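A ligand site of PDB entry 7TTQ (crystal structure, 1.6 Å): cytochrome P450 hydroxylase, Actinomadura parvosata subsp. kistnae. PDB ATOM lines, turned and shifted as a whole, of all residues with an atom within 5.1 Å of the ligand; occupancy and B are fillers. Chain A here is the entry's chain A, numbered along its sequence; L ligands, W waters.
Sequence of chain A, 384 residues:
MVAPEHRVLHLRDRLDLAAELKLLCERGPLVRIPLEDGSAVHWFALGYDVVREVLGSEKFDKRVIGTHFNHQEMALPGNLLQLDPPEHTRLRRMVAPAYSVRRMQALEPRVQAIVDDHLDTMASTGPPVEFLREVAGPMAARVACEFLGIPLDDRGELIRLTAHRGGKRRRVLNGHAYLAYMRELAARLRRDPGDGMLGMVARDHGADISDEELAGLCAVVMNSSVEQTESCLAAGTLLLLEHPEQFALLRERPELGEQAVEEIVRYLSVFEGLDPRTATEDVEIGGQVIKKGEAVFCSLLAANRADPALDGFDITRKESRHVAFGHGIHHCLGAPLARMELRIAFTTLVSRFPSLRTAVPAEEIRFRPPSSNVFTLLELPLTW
A ring nitrogen (NE2) of His 88 lies within hydrogen-bond range of an oxygen (O3) of the ligand. ND1 of His 330 lies within hydrogen-bond range of O4 of the ligand, at 2.6 Å. An iron atom (FE1) of the ligand is bound by the side-chain sulfur of Cys 332 (2.3 Å). An oxygen (O2) of the ligand lies within salt-bridge range of the guanidinium group (NH1) of Arg 277 (2.8 Å). O4 of the ligand sits close to N of Leu 81 (3.4 Å). NH1 of Arg 92 lies within salt-bridge range of O3 of the ligand.
N of Ser 225 sits at hydrogen-bond distance from O of Val 220 (3.0 Å). A ring nitrogen (NE2) of His 88 lies within hydrogen-bond range of a ring nitrogen (ND1) of His 330 (3.4 Å). The backbone carbonyl oxygen (O) of Asp 275 lies within hydrogen-bond range of the guanidinium group (NH1) of Arg 277, at 3.2 Å. The guanidinium group (NH1) of Arg 92 is in hydrogen-bond range of the backbone carbonyl oxygen (O) of His 331. O of Ile 329 is in hydrogen-bond range of NH1 of Arg 92. O of Gln 228 sits at hydrogen-bond distance from SG of Cys 232 (3.5 Å). N of Cys 332 is in hydrogen-bond range of O of Phe 325 (2.9 Å). The side-chain sulfur of Cys 332 sits close to the backbone NH of Gly 334 (3.3 Å).
O of Leu 80 sits close to O4 of the ligand, 3.4 Å away. Tyr 99 touches the ligand (OH to C26, 3.7 Å). Val 221 touches the ligand. Ser 225 touches the ligand. CB of Gln 228 touches C15 of the ligand (3.5 Å). Thr 229 touches the ligand. Cys 232 touches the ligand (SG to C19, 3.2 Å). Val 270 touches the ligand. CD2 of Phe 271 touches C2 of the ligand, at 3.6 Å. Leu 274 touches the ligand. Leu 300 touches the ligand (CD1 to C9, 3.6 Å). O of Ala 324 touches C9 of the ligand (3.5 Å). C of Phe 325 touches C9 of the ligand (3.4 Å). Gly 326 touches the ligand (N to C9, 3.6 Å). O of Ile 329 touches O3 of the ligand (3.6 Å). Leu 333 touches the ligand. Gly 334 touches the ligand. Leu 337 touches the ligand (CD2 to C26, 3.9 Å). Hydrophobic or aromatic side chains that line the ligand: Leu 80, Leu 81, His 88, Tyr 99, Val 221, Val 270, Phe 271, Leu 274, Leu 300, Phe 325, His 330, Leu 333 and Leu 337. Of the 34 residues printed, 24 come within 4 Å of the ligand. The nearest printed residue that does not touch the ligand is Ala 338 (4.04 Å).
Water W3 lies within hydrogen-bond range of O2 of the ligand (2.7 Å) and N of Asp 275 (2.8 Å). Water W2 bridges OG1 of Thr 229 (2.9 Å) and OG of Ser 225 (3.0 Å).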
ATOM      1  N   LEU A  55      13.995   0.369   2.052  1.00  0.00           N
ATOM      2  CA  LEU A  55      14.572   0.601   3.361  1.00  0.00           C
ATOM      3  C   LEU A  55      15.662  -0.416   3.680  1.00  0.00           C
ATOM      4  O   LEU A  55      16.554  -0.120   4.487  1.00  0.00           O
ATOM      5  CB  LEU A  55      13.490   0.545   4.442  1.00  0.00           C
ATOM      6  CG  LEU A  55      12.514   1.720   4.438  1.00  0.00           C
ATOM      7  CD1 LEU A  55      11.424   1.576   5.473  1.00  0.00           C
ATOM      8  CD2 LEU A  55      13.241   3.068   4.659  1.00  0.00           C
ATOM      9  N   LYS A  62      20.629   8.975   3.609  1.00  0.00           N
ATOM     10  CA  LYS A  62      19.684   9.925   4.164  1.00  0.00           C
ATOM     11  C   LYS A  62      20.188  11.354   4.023  1.00  0.00           C
ATOM     12  O   LYS A  62      20.104  12.176   4.968  1.00  0.00           O
ATOM     13  CB  LYS A  62      19.350   9.617   5.619  1.00  0.00           C
ATOM     14  CG  LYS A  62      18.560   8.351   5.741  1.00  0.00           C
ATOM     15  CD  LYS A  62      18.071   8.098   7.168  1.00  0.00           C
ATOM     16  CE  LYS A  62      16.788   8.841   7.499  1.00  0.00           C
ATOM     17  NZ  LYS A  62      16.949  10.289   7.777  1.00  0.00           N
ATOM     18  N   LEU A  80      20.493   9.305  15.770  1.00  0.00           N
ATOM     19  CA  LEU A  80      20.758   8.178  14.897  1.00  0.00           C
ATOM     20  C   LEU A  80      20.065   8.304  13.560  1.00  0.00           C
ATOM     21  O   LEU A  80      20.597   7.853  12.540  1.00  0.00           O
ATOM     22  CB  LEU A  80      20.312   6.868  15.564  1.00  0.00           C
ATOM     23  CG  LEU A  80      21.225   6.231  16.577  1.00  0.00           C
ATOM     24  CD1 LEU A  80      20.430   5.169  17.345  1.00  0.00           C
ATOM     25  CD2 LEU A  80      22.444   5.627  15.900  1.00  0.00           C
ATOM     26  N   LEU A  81      18.878   8.900  13.531  1.00  0.00           N
ATOM     27  CA  LEU A  81      18.103   8.900  12.297  1.00  0.00           C
ATOM     28  C   LEU A  81      18.752   9.755  11.221  1.00  0.00           C
ATOM     29  O   LEU A  81      18.443   9.584  10.039  1.00  0.00           O
ATOM     30  CB  LEU A  81      16.701   9.388  12.573  1.00  0.00           C
ATOM     31  CG  LEU A  81      15.628   9.053  11.546  1.00  0.00           C
ATOM     32  CD1 LEU A  81      15.718   7.619  11.031  1.00  0.00           C
ATOM     33  CD2 LEU A  81      14.274   9.307  12.201  1.00  0.00           C
ATOM     34  N   HIS A  88      26.605   5.690  11.863  1.00  0.00           N
ATOM     35  CA  HIS A  88      25.336   5.159  12.351  1.00  0.00           C
ATOM     36  C   HIS A  88      25.549   3.837  13.068  1.00  0.00           C
ATOM     37  O   HIS A  88      25.034   3.619  14.186  1.00  0.00           O
ATOM     38  CB  HIS A  88      24.365   4.986  11.191  1.00  0.00           C
ATOM     39  CG  HIS A  88      23.116   4.271  11.582  1.00  0.00           C
ATOM     40  ND1 HIS A  88      22.957   2.908  11.479  1.00  0.00           N
ATOM     41  CD2 HIS A  88      21.980   4.747  12.151  1.00  0.00           C
ATOM     42  CE1 HIS A  88      21.772   2.569  11.934  1.00  0.00           C
ATOM     43  NE2 HIS A  88      21.147   3.662  12.322  1.00  0.00           N
ATOM     44  N   ARG A  92      24.796   3.203  16.989  1.00  0.00           N
ATOM     45  CA  ARG A  92      23.684   2.318  17.314  1.00  0.00           C
ATOM     46  C   ARG A  92      24.169   1.093  18.083  1.00  0.00           C
ATOM     47  O   ARG A  92      23.471   0.611  18.981  1.00  0.00           O
ATOM     48  CB  ARG A  92      22.917   1.923  16.060  1.00  0.00           C
ATOM     49  CG  ARG A  92      21.737   1.041  16.392  1.00  0.00           C
ATOM     50  CD  ARG A  92      20.605   1.166  15.419  1.00  0.00           C
ATOM     51  NE  ARG A  92      19.558   0.229  15.809  1.00  0.00           N
ATOM     52  CZ  ARG A  92      18.312   0.292  15.374  1.00  0.00           C
ATOM     53  NH1 ARG A  92      17.885   1.294  14.643  1.00  0.00           N
ATOM     54  NH2 ARG A  92      17.460  -0.653  15.763  1.00  0.00           N
ATOM     55  N   TYR A  99      17.999  -1.919  24.890  1.00  0.00           N
ATOM     56  CA  TYR A  99      16.689  -2.439  24.496  1.00  0.00           C
ATOM     57  C   TYR A  99      16.641  -3.963  24.334  1.00  0.00           C
ATOM     58  O   TYR A  99      15.643  -4.504  23.833  1.00  0.00           O
ATOM     59  CB  TYR A  99      16.187  -1.797  23.194  1.00  0.00           C
ATOM     60  CG  TYR A  99      16.186  -0.279  23.145  1.00  0.00           C
ATOM     61  CD1 TYR A  99      17.355   0.443  22.934  1.00  0.00           C
ATOM     62  CD2 TYR A  99      15.004   0.440  23.331  1.00  0.00           C
ATOM     63  CE1 TYR A  99      17.359   1.828  22.902  1.00  0.00           C
ATOM     64  CE2 TYR A  99      14.996   1.830  23.303  1.00  0.00           C
ATOM     65  CZ  TYR A  99      16.166   2.512  23.068  1.00  0.00           C
ATOM     66  OH  TYR A  99      16.181   3.877  23.043  1.00  0.00           O
ATOM     67  N   PHE A 147      12.876   4.613  31.653  1.00  0.00           N
ATOM     68  CA  PHE A 147      13.750   3.945  30.714  1.00  0.00           C
ATOM     69  C   PHE A 147      15.122   4.612  30.656  1.00  0.00           C
ATOM     70  O   PHE A 147      16.156   3.926  30.655  1.00  0.00           O
ATOM     71  CB  PHE A 147      13.125   3.947  29.311  1.00  0.00           C
ATOM     72  CG  PHE A 147      14.069   3.492  28.254  1.00  0.00           C
ATOM     73  CD1 PHE A 147      14.445   2.164  28.206  1.00  0.00           C
ATOM     74  CD2 PHE A 147      14.623   4.394  27.363  1.00  0.00           C
ATOM     75  CE1 PHE A 147      15.338   1.712  27.254  1.00  0.00           C
ATOM     76  CE2 PHE A 147      15.552   3.937  26.431  1.00  0.00           C
ATOM     77  CZ  PHE A 147      15.879   2.618  26.367  1.00  0.00           C
ATOM     78  N   VAL A 220      15.848  12.679  21.798  1.00  0.00           N
ATOM     79  CA  VAL A 220      15.032  11.900  20.869  1.00  0.00           C
ATOM     80  C   VAL A 220      14.046  11.041  21.645  1.00  0.00           C
ATOM     81  O   VAL A 220      12.867  10.930  21.270  1.00  0.00           O
ATOM     82  CB  VAL A 220      15.950  11.058  19.967  1.00  0.00           C
ATOM     83  CG1 VAL A 220      15.106  10.109  19.119  1.00  0.00           C
ATOM     84  CG2 VAL A 220      16.785  12.013  19.058  1.00  0.00           C
ATOM     85  N   VAL A 221      14.494  10.434  22.744  1.00  0.00           N
ATOM     86  CA  VAL A 221      13.587   9.606  23.532  1.00  0.00           C
ATOM     87  C   VAL A 221      12.493  10.470  24.160  1.00  0.00           C
ATOM     88  O   VAL A 221      11.324  10.064  24.190  1.00  0.00           O
ATOM     89  CB  VAL A 221      14.362   8.822  24.600  1.00  0.00           C
ATOM     90  CG1 VAL A 221      13.400   8.055  25.491  1.00  0.00           C
ATOM     91  CG2 VAL A 221      15.325   7.854  24.001  1.00  0.00           C
ATOM     92  N   SER A 225       9.972  10.631  20.455  1.00  0.00           N
ATOM     93  CA  SER A 225       9.511   9.285  20.777  1.00  0.00           C
ATOM     94  C   SER A 225       8.266   9.352  21.636  1.00  0.00           C
ATOM     95  O   SER A 225       7.291   8.616  21.398  1.00  0.00           O
ATOM     96  CB  SER A 225      10.633   8.496  21.470  1.00  0.00           C
ATOM     97  OG  SER A 225      10.425   8.326  22.871  1.00  0.00           O
ATOM     98  N   GLN A 228       5.281  10.082  19.365  1.00  0.00           N
ATOM     99  CA  GLN A 228       4.742   8.892  18.702  1.00  0.00           C
ATOM    100  C   GLN A 228       3.941   8.044  19.694  1.00  0.00           C
ATOM    101  O   GLN A 228       2.871   7.533  19.374  1.00  0.00           O
ATOM    102  CB  GLN A 228       5.845   8.023  18.107  1.00  0.00           C
ATOM    103  CG  GLN A 228       6.999   8.685  17.439  1.00  0.00           C
ATOM    104  CD  GLN A 228       6.590   9.540  16.326  1.00  0.00           C
ATOM    105  OE1 GLN A 228       6.906  10.730  16.308  1.00  0.00           O
ATOM    106  NE2 GLN A 228       5.930   8.962  15.339  1.00  0.00           N
ATOM    107  N   THR A 229       4.533   7.808  20.869  1.00  0.00           N
ATOM    108  CA  THR A 229       3.980   6.874  21.822  1.00  0.00           C
ATOM    109  C   THR A 229       2.679   7.420  22.387  1.00  0.00           C
ATOM    110  O   THR A 229       1.672   6.713  22.452  1.00  0.00           O
ATOM    111  CB  THR A 229       4.972   6.600  22.941  1.00  0.00           C
ATOM    112  OG1 THR A 229       6.217   6.122  22.395  1.00  0.00           O
ATOM    113  CG2 THR A 229       4.417   5.549  23.897  1.00  0.00           C
ATOM    114  N   CYS A 232      -0.038   7.058  19.790  1.00  0.00           N
ATOM    115  CA  CYS A 232      -0.541   5.685  19.776  1.00  0.00           C
ATOM    116  C   CYS A 232      -1.471   5.416  20.955  1.00  0.00           C
ATOM    117  O   CYS A 232      -2.523   4.781  20.782  1.00  0.00           O
ATOM    118  CB  CYS A 232       0.641   4.699  19.790  1.00  0.00           C
ATOM    119  SG  CYS A 232       1.470   4.552  18.208  1.00  0.00           S
ATOM    120  N   VAL A 265      -0.767  -0.296  15.894  1.00  0.00           N
ATOM    121  CA  VAL A 265       0.254   0.553  15.282  1.00  0.00           C
ATOM    122  C   VAL A 265       0.152   0.503  13.756  1.00  0.00           C
ATOM    123  O   VAL A 265       0.362   1.531  13.093  1.00  0.00           O
ATOM    124  CB  VAL A 265       1.693   0.216  15.747  1.00  0.00           C
ATOM    125  CG1 VAL A 265       1.883   0.434  17.259  1.00  0.00           C
ATOM    126  CG2 VAL A 265       2.110  -1.183  15.351  1.00  0.00           C
ATOM    127  N   VAL A 270       1.083   6.261  12.986  1.00  0.00           N
ATOM    128  CA  VAL A 270       1.252   7.621  13.485  1.00  0.00           C
ATOM    129  C   VAL A 270       2.480   8.306  12.871  1.00  0.00           C
ATOM    130  O   VAL A 270       2.517   9.535  12.731  1.00  0.00           O
ATOM    131  CB  VAL A 270       1.332   7.700  15.033  1.00  0.00           C
ATOM    132  CG1 VAL A 270       0.038   7.179  15.645  1.00  0.00           C
ATOM    133  CG2 VAL A 270       2.586   6.995  15.530  1.00  0.00           C
ATOM    134  N   PHE A 271       3.523   7.539  12.555  1.00  0.00           N
ATOM    135  CA  PHE A 271       4.653   7.978  11.772  1.00  0.00           C
ATOM    136  C   PHE A 271       4.274   7.654  10.329  1.00  0.00           C
ATOM    137  O   PHE A 271       4.353   6.509   9.893  1.00  0.00           O
ATOM    138  CB  PHE A 271       5.916   7.254  12.222  1.00  0.00           C
ATOM    139  CG  PHE A 271       7.203   7.902  11.829  1.00  0.00           C
ATOM    140  CD1 PHE A 271       7.346   8.604  10.651  1.00  0.00           C
ATOM    141  CD2 PHE A 271       8.296   7.808  12.672  1.00  0.00           C
ATOM    142  CE1 PHE A 271       8.577   9.184  10.306  1.00  0.00           C
ATOM    143  CE2 PHE A 271       9.513   8.385  12.337  1.00  0.00           C
ATOM    144  CZ  PHE A 271       9.642   9.083  11.168  1.00  0.00           C
ATOM    145  N   LEU A 274       8.392   8.657   5.747  1.00  0.00           N
ATOM    146  CA  LEU A 274       9.775   8.734   6.157  1.00  0.00           C
ATOM    147  C   LEU A 274      10.559   9.837   5.434  1.00  0.00           C
ATOM    148  O   LEU A 274      10.210  10.259   4.313  1.00  0.00           O
ATOM    149  CB  LEU A 274      10.431   7.381   5.912  1.00  0.00           C
ATOM    150  CG  LEU A 274       9.843   6.220   6.723  1.00  0.00           C
ATOM    151  CD1 LEU A 274      10.720   5.027   6.540  1.00  0.00           C
ATOM    152  CD2 LEU A 274       9.685   6.608   8.210  1.00  0.00           C
ATOM    153  N   ASP A 275      11.658  10.248   6.095  1.00  0.00           N
ATOM    154  CA  ASP A 275      12.660  11.097   5.476  1.00  0.00           C
ATOM    155  C   ASP A 275      13.096  10.482   4.153  1.00  0.00           C
ATOM    156  O   ASP A 275      13.202   9.251   4.060  1.00  0.00           O
ATOM    157  CB  ASP A 275      13.922  11.187   6.368  1.00  0.00           C
ATOM    158  CG  ASP A 275      13.710  11.830   7.718  1.00  0.00           C
ATOM    159  OD1 ASP A 275      12.846  12.715   7.849  1.00  0.00           O
ATOM    160  OD2 ASP A 275      14.500  11.472   8.651  1.00  0.00           O
ATOM    161  N   ARG A 277      15.078   8.888   1.068  1.00  0.00           N
ATOM    162  CA  ARG A 277      16.265   8.110   0.770  1.00  0.00           C
ATOM    163  C   ARG A 277      16.715   8.469  -0.631  1.00  0.00           C
ATOM    164  O   ARG A 277      15.921   8.346  -1.592  1.00  0.00           O
ATOM    165  CB  ARG A 277      15.962   6.615   0.877  1.00  0.00           C
ATOM    166  CG  ARG A 277      16.221   5.955   2.202  1.00  0.00           C
ATOM    167  CD  ARG A 277      15.524   6.606   3.386  1.00  0.00           C
ATOM    168  NE  ARG A 277      15.761   5.792   4.576  1.00  0.00           N
ATOM    169  CZ  ARG A 277      15.128   5.936   5.727  1.00  0.00           C
ATOM    170  NH1 ARG A 277      14.206   6.867   5.917  1.00  0.00           N
ATOM    171  NH2 ARG A 277      15.428   5.091   6.733  1.00  0.00           N
ATOM    172  N   LEU A 300       4.683   4.871   5.039  1.00  0.00           N
ATOM    173  CA  LEU A 300       4.264   3.804   5.949  1.00  0.00           C
ATOM    174  C   LEU A 300       2.754   3.725   6.016  1.00  0.00           C
ATOM    175  O   LEU A 300       2.163   2.644   6.083  1.00  0.00           O
ATOM    176  CB  LEU A 300       4.867   4.065   7.327  1.00  0.00           C
ATOM    177  CG  LEU A 300       6.377   4.254   7.378  1.00  0.00           C
ATOM    178  CD1 LEU A 300       6.904   4.283   8.806  1.00  0.00           C
ATOM    179  CD2 LEU A 300       7.125   3.180   6.576  1.00  0.00           C
ATOM    180  N   VAL A 323       4.743  -1.934   8.426  1.00  0.00           N
ATOM    181  CA  VAL A 323       6.055  -1.307   8.537  1.00  0.00           C
ATOM    182  C   VAL A 323       5.982  -0.070   9.443  1.00  0.00           C
ATOM    183  O   VAL A 323       6.695   0.905   9.219  1.00  0.00           O
ATOM    184  CB  VAL A 323       6.587  -0.913   7.135  1.00  0.00           C
ATOM    185  CG1 VAL A 323       7.117  -2.134   6.405  1.00  0.00           C
ATOM    186  CG2 VAL A 323       5.499  -0.198   6.315  1.00  0.00           C
ATOM    187  N   ALA A 324       5.133  -0.133  10.476  1.00  0.00           N
ATOM    188  CA  ALA A 324       4.903   1.038  11.333  1.00  0.00           C
ATOM    189  C   ALA A 324       6.146   1.511  12.053  1.00  0.00           C
ATOM    190  O   ALA A 324       6.199   2.696  12.416  1.00  0.00           O
ATOM    191  CB  ALA A 324       3.781   0.741  12.344  1.00  0.00           C
ATOM    192  N   PHE A 325       7.138   0.629  12.262  1.00  0.00           N
ATOM    193  CA  PHE A 325       8.405   0.917  12.901  1.00  0.00           C
ATOM    194  C   PHE A 325       9.561   0.966  11.884  1.00  0.00           C
ATOM    195  O   PHE A 325      10.739   0.963  12.286  1.00  0.00           O
ATOM    196  CB  PHE A 325       8.718  -0.101  13.994  1.00  0.00           C
ATOM    197  CG  PHE A 325       7.802  -0.049  15.176  1.00  0.00           C
ATOM    198  CD1 PHE A 325       7.867   0.985  16.077  1.00  0.00           C
ATOM    199  CD2 PHE A 325       6.942  -1.096  15.439  1.00  0.00           C
ATOM    200  CE1 PHE A 325       7.062   1.028  17.197  1.00  0.00           C
ATOM    201  CE2 PHE A 325       6.126  -1.087  16.538  1.00  0.00           C
ATOM    202  CZ  PHE A 325       6.154  -0.026  17.417  1.00  0.00           C
ATOM    203  N   GLY A 326       9.268   0.953  10.598  1.00  0.00           N
ATOM    204  CA  GLY A 326      10.321   0.953   9.608  1.00  0.00           C
ATOM    205  C   GLY A 326      10.885  -0.435   9.360  1.00  0.00           C
ATOM    206  O   GLY A 326      10.230  -1.446   9.636  1.00  0.00           O
ATOM    207  N   ILE A 329      18.380  -0.887   8.685  1.00  0.00           N
ATOM    208  CA  ILE A 329      19.332  -0.458   9.698  1.00  0.00           C
ATOM    209  C   ILE A 329      18.764   0.637  10.615  1.00  0.00           C
ATOM    210  O   ILE A 329      19.230   0.781  11.756  1.00  0.00           O
ATOM    211  CB  ILE A 329      20.677  -0.017   9.085  1.00  0.00           C
ATOM    212  CG1 ILE A 329      20.539   1.234   8.217  1.00  0.00           C
ATOM    213  CG2 ILE A 329      21.322  -1.171   8.320  1.00  0.00           C
ATOM    214  CD1 ILE A 329      21.899   1.880   7.857  1.00  0.00           C
ATOM    215  N   HIS A 330      17.754   1.381  10.146  1.00  0.00           N
ATOM    216  CA  HIS A 330      17.149   2.455  10.907  1.00  0.00           C
ATOM    217  C   HIS A 330      15.841   2.033  11.560  1.00  0.00           C
ATOM    218  O   HIS A 330      15.162   2.893  12.114  1.00  0.00           O
ATOM    219  CB  HIS A 330      16.882   3.693  10.043  1.00  0.00           C
ATOM    220  CG  HIS A 330      18.115   4.406   9.607  1.00  0.00           C
ATOM    221  ND1 HIS A 330      18.830   5.242  10.451  1.00  0.00           N
ATOM    222  CD2 HIS A 330      18.767   4.430   8.424  1.00  0.00           C
ATOM    223  CE1 HIS A 330      19.863   5.753   9.796  1.00  0.00           C
ATOM    224  NE2 HIS A 330      19.864   5.258   8.574  1.00  0.00           N
ATOM    225  N   HIS A 331      15.463   0.734  11.484  1.00  0.00           N
ATOM    226  CA  HIS A 331      14.286   0.223  12.180  1.00  0.00           C
ATOM    227  C   HIS A 331      14.244   0.770  13.607  1.00  0.00           C
ATOM    228  O   HIS A 331      15.230   0.733  14.324  1.00  0.00           O
ATOM    229  CB  HIS A 331      14.323  -1.318  12.221  1.00  0.00           C
ATOM    230  CG  HIS A 331      13.130  -1.939  12.870  1.00  0.00           C
ATOM    231  ND1 HIS A 331      13.132  -2.372  14.171  1.00  0.00           N
ATOM    232  CD2 HIS A 331      11.895  -2.247  12.375  1.00  0.00           C
ATOM    233  CE1 HIS A 331      11.955  -2.893  14.472  1.00  0.00           C
ATOM    234  NE2 HIS A 331      11.180  -2.841  13.396  1.00  0.00           N
ATOM    235  N   CYS A 332      13.053   1.215  14.018  1.00  0.00           N
ATOM    236  CA  CYS A 332      12.916   1.889  15.302  1.00  0.00           C
ATOM    237  C   CYS A 332      13.658   1.189  16.439  1.00  0.00           C
ATOM    238  O   CYS A 332      13.370   0.052  16.795  1.00  0.00           O
ATOM    239  CB  CYS A 332      11.427   1.984  15.671  1.00  0.00           C
ATOM    240  SG  CYS A 332      11.105   2.828  17.235  1.00  0.00           S
ATOM    241  N   LEU A 333      14.636   1.893  16.986  1.00  0.00           N
ATOM    242  CA  LEU A 333      15.412   1.391  18.104  1.00  0.00           C
ATOM    243  C   LEU A 333      14.540   1.216  19.334  1.00  0.00           C
ATOM    244  O   LEU A 333      14.774   0.314  20.156  1.00  0.00           O
ATOM    245  CB  LEU A 333      16.563   2.352  18.366  1.00  0.00           C
ATOM    246  CG  LEU A 333      17.572   1.999  19.456  1.00  0.00           C
ATOM    247  CD1 LEU A 333      18.392   0.799  19.059  1.00  0.00           C
ATOM    248  CD2 LEU A 333      18.458   3.234  19.708  1.00  0.00           C
ATOM    249  N   GLY A 334      13.484   2.021  19.423  1.00  0.00           N
ATOM    250  CA  GLY A 334      12.574   1.964  20.528  1.00  0.00           C
ATOM    251  C   GLY A 334      11.470   0.958  20.435  1.00  0.00           C
ATOM    252  O   GLY A 334      10.658   0.888  21.372  1.00  0.00           O
ATOM    253  N   LEU A 337      10.515  -1.122  23.541  1.00  0.00           N
ATOM    254  CA  LEU A 337       9.897  -0.336  24.599  1.00  0.00           C
ATOM    255  C   LEU A 337       8.497   0.059  24.216  1.00  0.00           C
ATOM    256  O   LEU A 337       7.567  -0.089  25.000  1.00  0.00           O
ATOM    257  CB  LEU A 337      10.733   0.894  24.925  1.00  0.00           C
ATOM    258  CG  LEU A 337      10.201   1.777  26.045  1.00  0.00           C
ATOM    259  CD1 LEU A 337      10.021   0.956  27.290  1.00  0.00           C
ATOM    260  CD2 LEU A 337      11.126   2.924  26.298  1.00  0.00           C
ATOM    261  N   ALA A 338       8.341   0.612  23.010  1.00  0.00           N
ATOM    262  CA  ALA A 338       7.002   1.008  22.549  1.00  0.00           C
ATOM    263  C   ALA A 338       6.021  -0.154  22.618  1.00  0.00           C
ATOM    264  O   ALA A 338       4.878   0.014  23.075  1.00  0.00           O
ATOM    265  CB  ALA A 338       7.070   1.554  21.123  1.00  0.00           C
ATOM    266  N   LEU A 342       2.844   0.016  25.149  1.00  0.00           N
ATOM    267  CA  LEU A 342       1.502   0.015  24.587  1.00  0.00           C
ATOM    268  C   LEU A 342       0.696  -1.215  25.027  1.00  0.00           C
ATOM    269  O   LEU A 342      -0.492  -1.099  25.333  1.00  0.00           O
ATOM    270  CB  LEU A 342       1.552   0.083  23.059  1.00  0.00           C
ATOM    271  CG  LEU A 342       2.093   1.407  22.476  1.00  0.00           C
ATOM    272  CD1 LEU A 342       2.220   1.362  20.996  1.00  0.00           C
ATOM    273  CD2 LEU A 342       1.244   2.611  22.948  1.00  0.00           C
HETATM  274  C1  LIG L   1      13.299   5.211  14.332  1.00  0.00           C
HETATM  275  C2  LIG L   1       8.477   4.716  14.507  1.00  0.00           C
HETATM  276  C3  LIG L   1       8.623   4.970  19.343  1.00  0.00           C
HETATM  277  C4  LIG L   1      13.397   5.631  19.174  1.00  0.00           C
HETATM  278  C5  LIG L   1      11.996   4.984  13.970  1.00  0.00           C
HETATM  279  C6  LIG L   1      11.534   4.771  12.608  1.00  0.00           C
HETATM  280  C7  LIG L   1      10.199   4.631  12.678  1.00  0.00           C
HETATM  281  C8  LIG L   1       9.780   4.788  14.056  1.00  0.00           C
HETATM  282  C9  LIG L   1       9.165   4.375  11.560  1.00  0.00           C
HETATM  283  C10 LIG L   1      12.450   4.677  11.378  1.00  0.00           C
HETATM  284  C11 LIG L   1      12.497   6.008  10.626  1.00  0.00           C
HETATM  285  C12 LIG L   1      13.224   5.917   9.298  1.00  0.00           C
HETATM  286  O1  LIG L   1      13.752   4.823   8.996  1.00  0.00           O
HETATM  287  O2  LIG L   1      13.276   6.936   8.544  1.00  0.00           O
HETATM  288  C13 LIG L   1       8.103   4.723  15.827  1.00  0.00           C
HETATM  289  C14 LIG L   1       6.755   4.569  16.328  1.00  0.00           C
HETATM  290  C15 LIG L   1       6.830   4.649  17.666  1.00  0.00           C
HETATM  291  C16 LIG L   1       8.194   4.861  18.039  1.00  0.00           C
HETATM  292  C17 LIG L   1       5.518   4.334  15.458  1.00  0.00           C
HETATM  293  C18 LIG L   1       5.709   4.528  18.749  1.00  0.00           C
HETATM  294  C19 LIG L   1       4.559   3.904  18.551  1.00  0.00           C
HETATM  295  C20 LIG L   1       9.922   5.088  19.739  1.00  0.00           C
HETATM  296  C21 LIG L   1      10.433   5.091  21.102  1.00  0.00           C
HETATM  297  C22 LIG L   1      11.761   5.295  21.036  1.00  0.00           C
HETATM  298  C23 LIG L   1      12.118   5.405  19.652  1.00  0.00           C
HETATM  299  C24 LIG L   1       9.573   4.898  22.362  1.00  0.00           C
HETATM  300  C25 LIG L   1      12.856   5.354  22.123  1.00  0.00           C
HETATM  301  C26 LIG L   1      12.667   4.997  23.403  1.00  0.00           C
HETATM  302  C27 LIG L   1      13.773   5.632  17.848  1.00  0.00           C
HETATM  303  C28 LIG L   1      15.093   5.892  17.338  1.00  0.00           C
HETATM  304  C29 LIG L   1      15.097   5.766  16.002  1.00  0.00           C
HETATM  305  C30 LIG L   1      13.738   5.435  15.612  1.00  0.00           C
HETATM  306  C31 LIG L   1      16.270   6.240  18.259  1.00  0.00           C
HETATM  307  C32 LIG L   1      16.299   5.945  15.031  1.00  0.00           C
HETATM  308  C33 LIG L   1      16.989   4.600  14.808  1.00  0.00           C
HETATM  309  C34 LIG L   1      18.069   4.640  13.738  1.00  0.00           C
HETATM  310  O3  LIG L   1      18.948   3.741  13.739  1.00  0.00           O
HETATM  311  O4  LIG L   1      18.029   5.613  12.925  1.00  0.00           O
HETATM  312  N1  LIG L   1      10.907   5.008  14.798  1.00  0.00           N
HETATM  313  N2  LIG L   1       8.978   4.935  16.893  1.00  0.00           N
HETATM  314  N3  LIG L   1      10.977   5.318  18.889  1.00  0.00           N
HETATM  315  N4  LIG L   1      12.949   5.358  16.771  1.00  0.00           N
HETATM  316 FE1  LIG L   1      10.964   5.054  16.838  1.00  0.00          FE
HETATM  317  O   HOH W   1      13.438   2.179   8.902  1.00  0.00           O
HETATM  318  O   HOH W   2       8.078   7.125  24.338  1.00  0.00           O
HETATM  319  O   HOH W   3      12.099   9.405   8.729  1.00  0.00           O
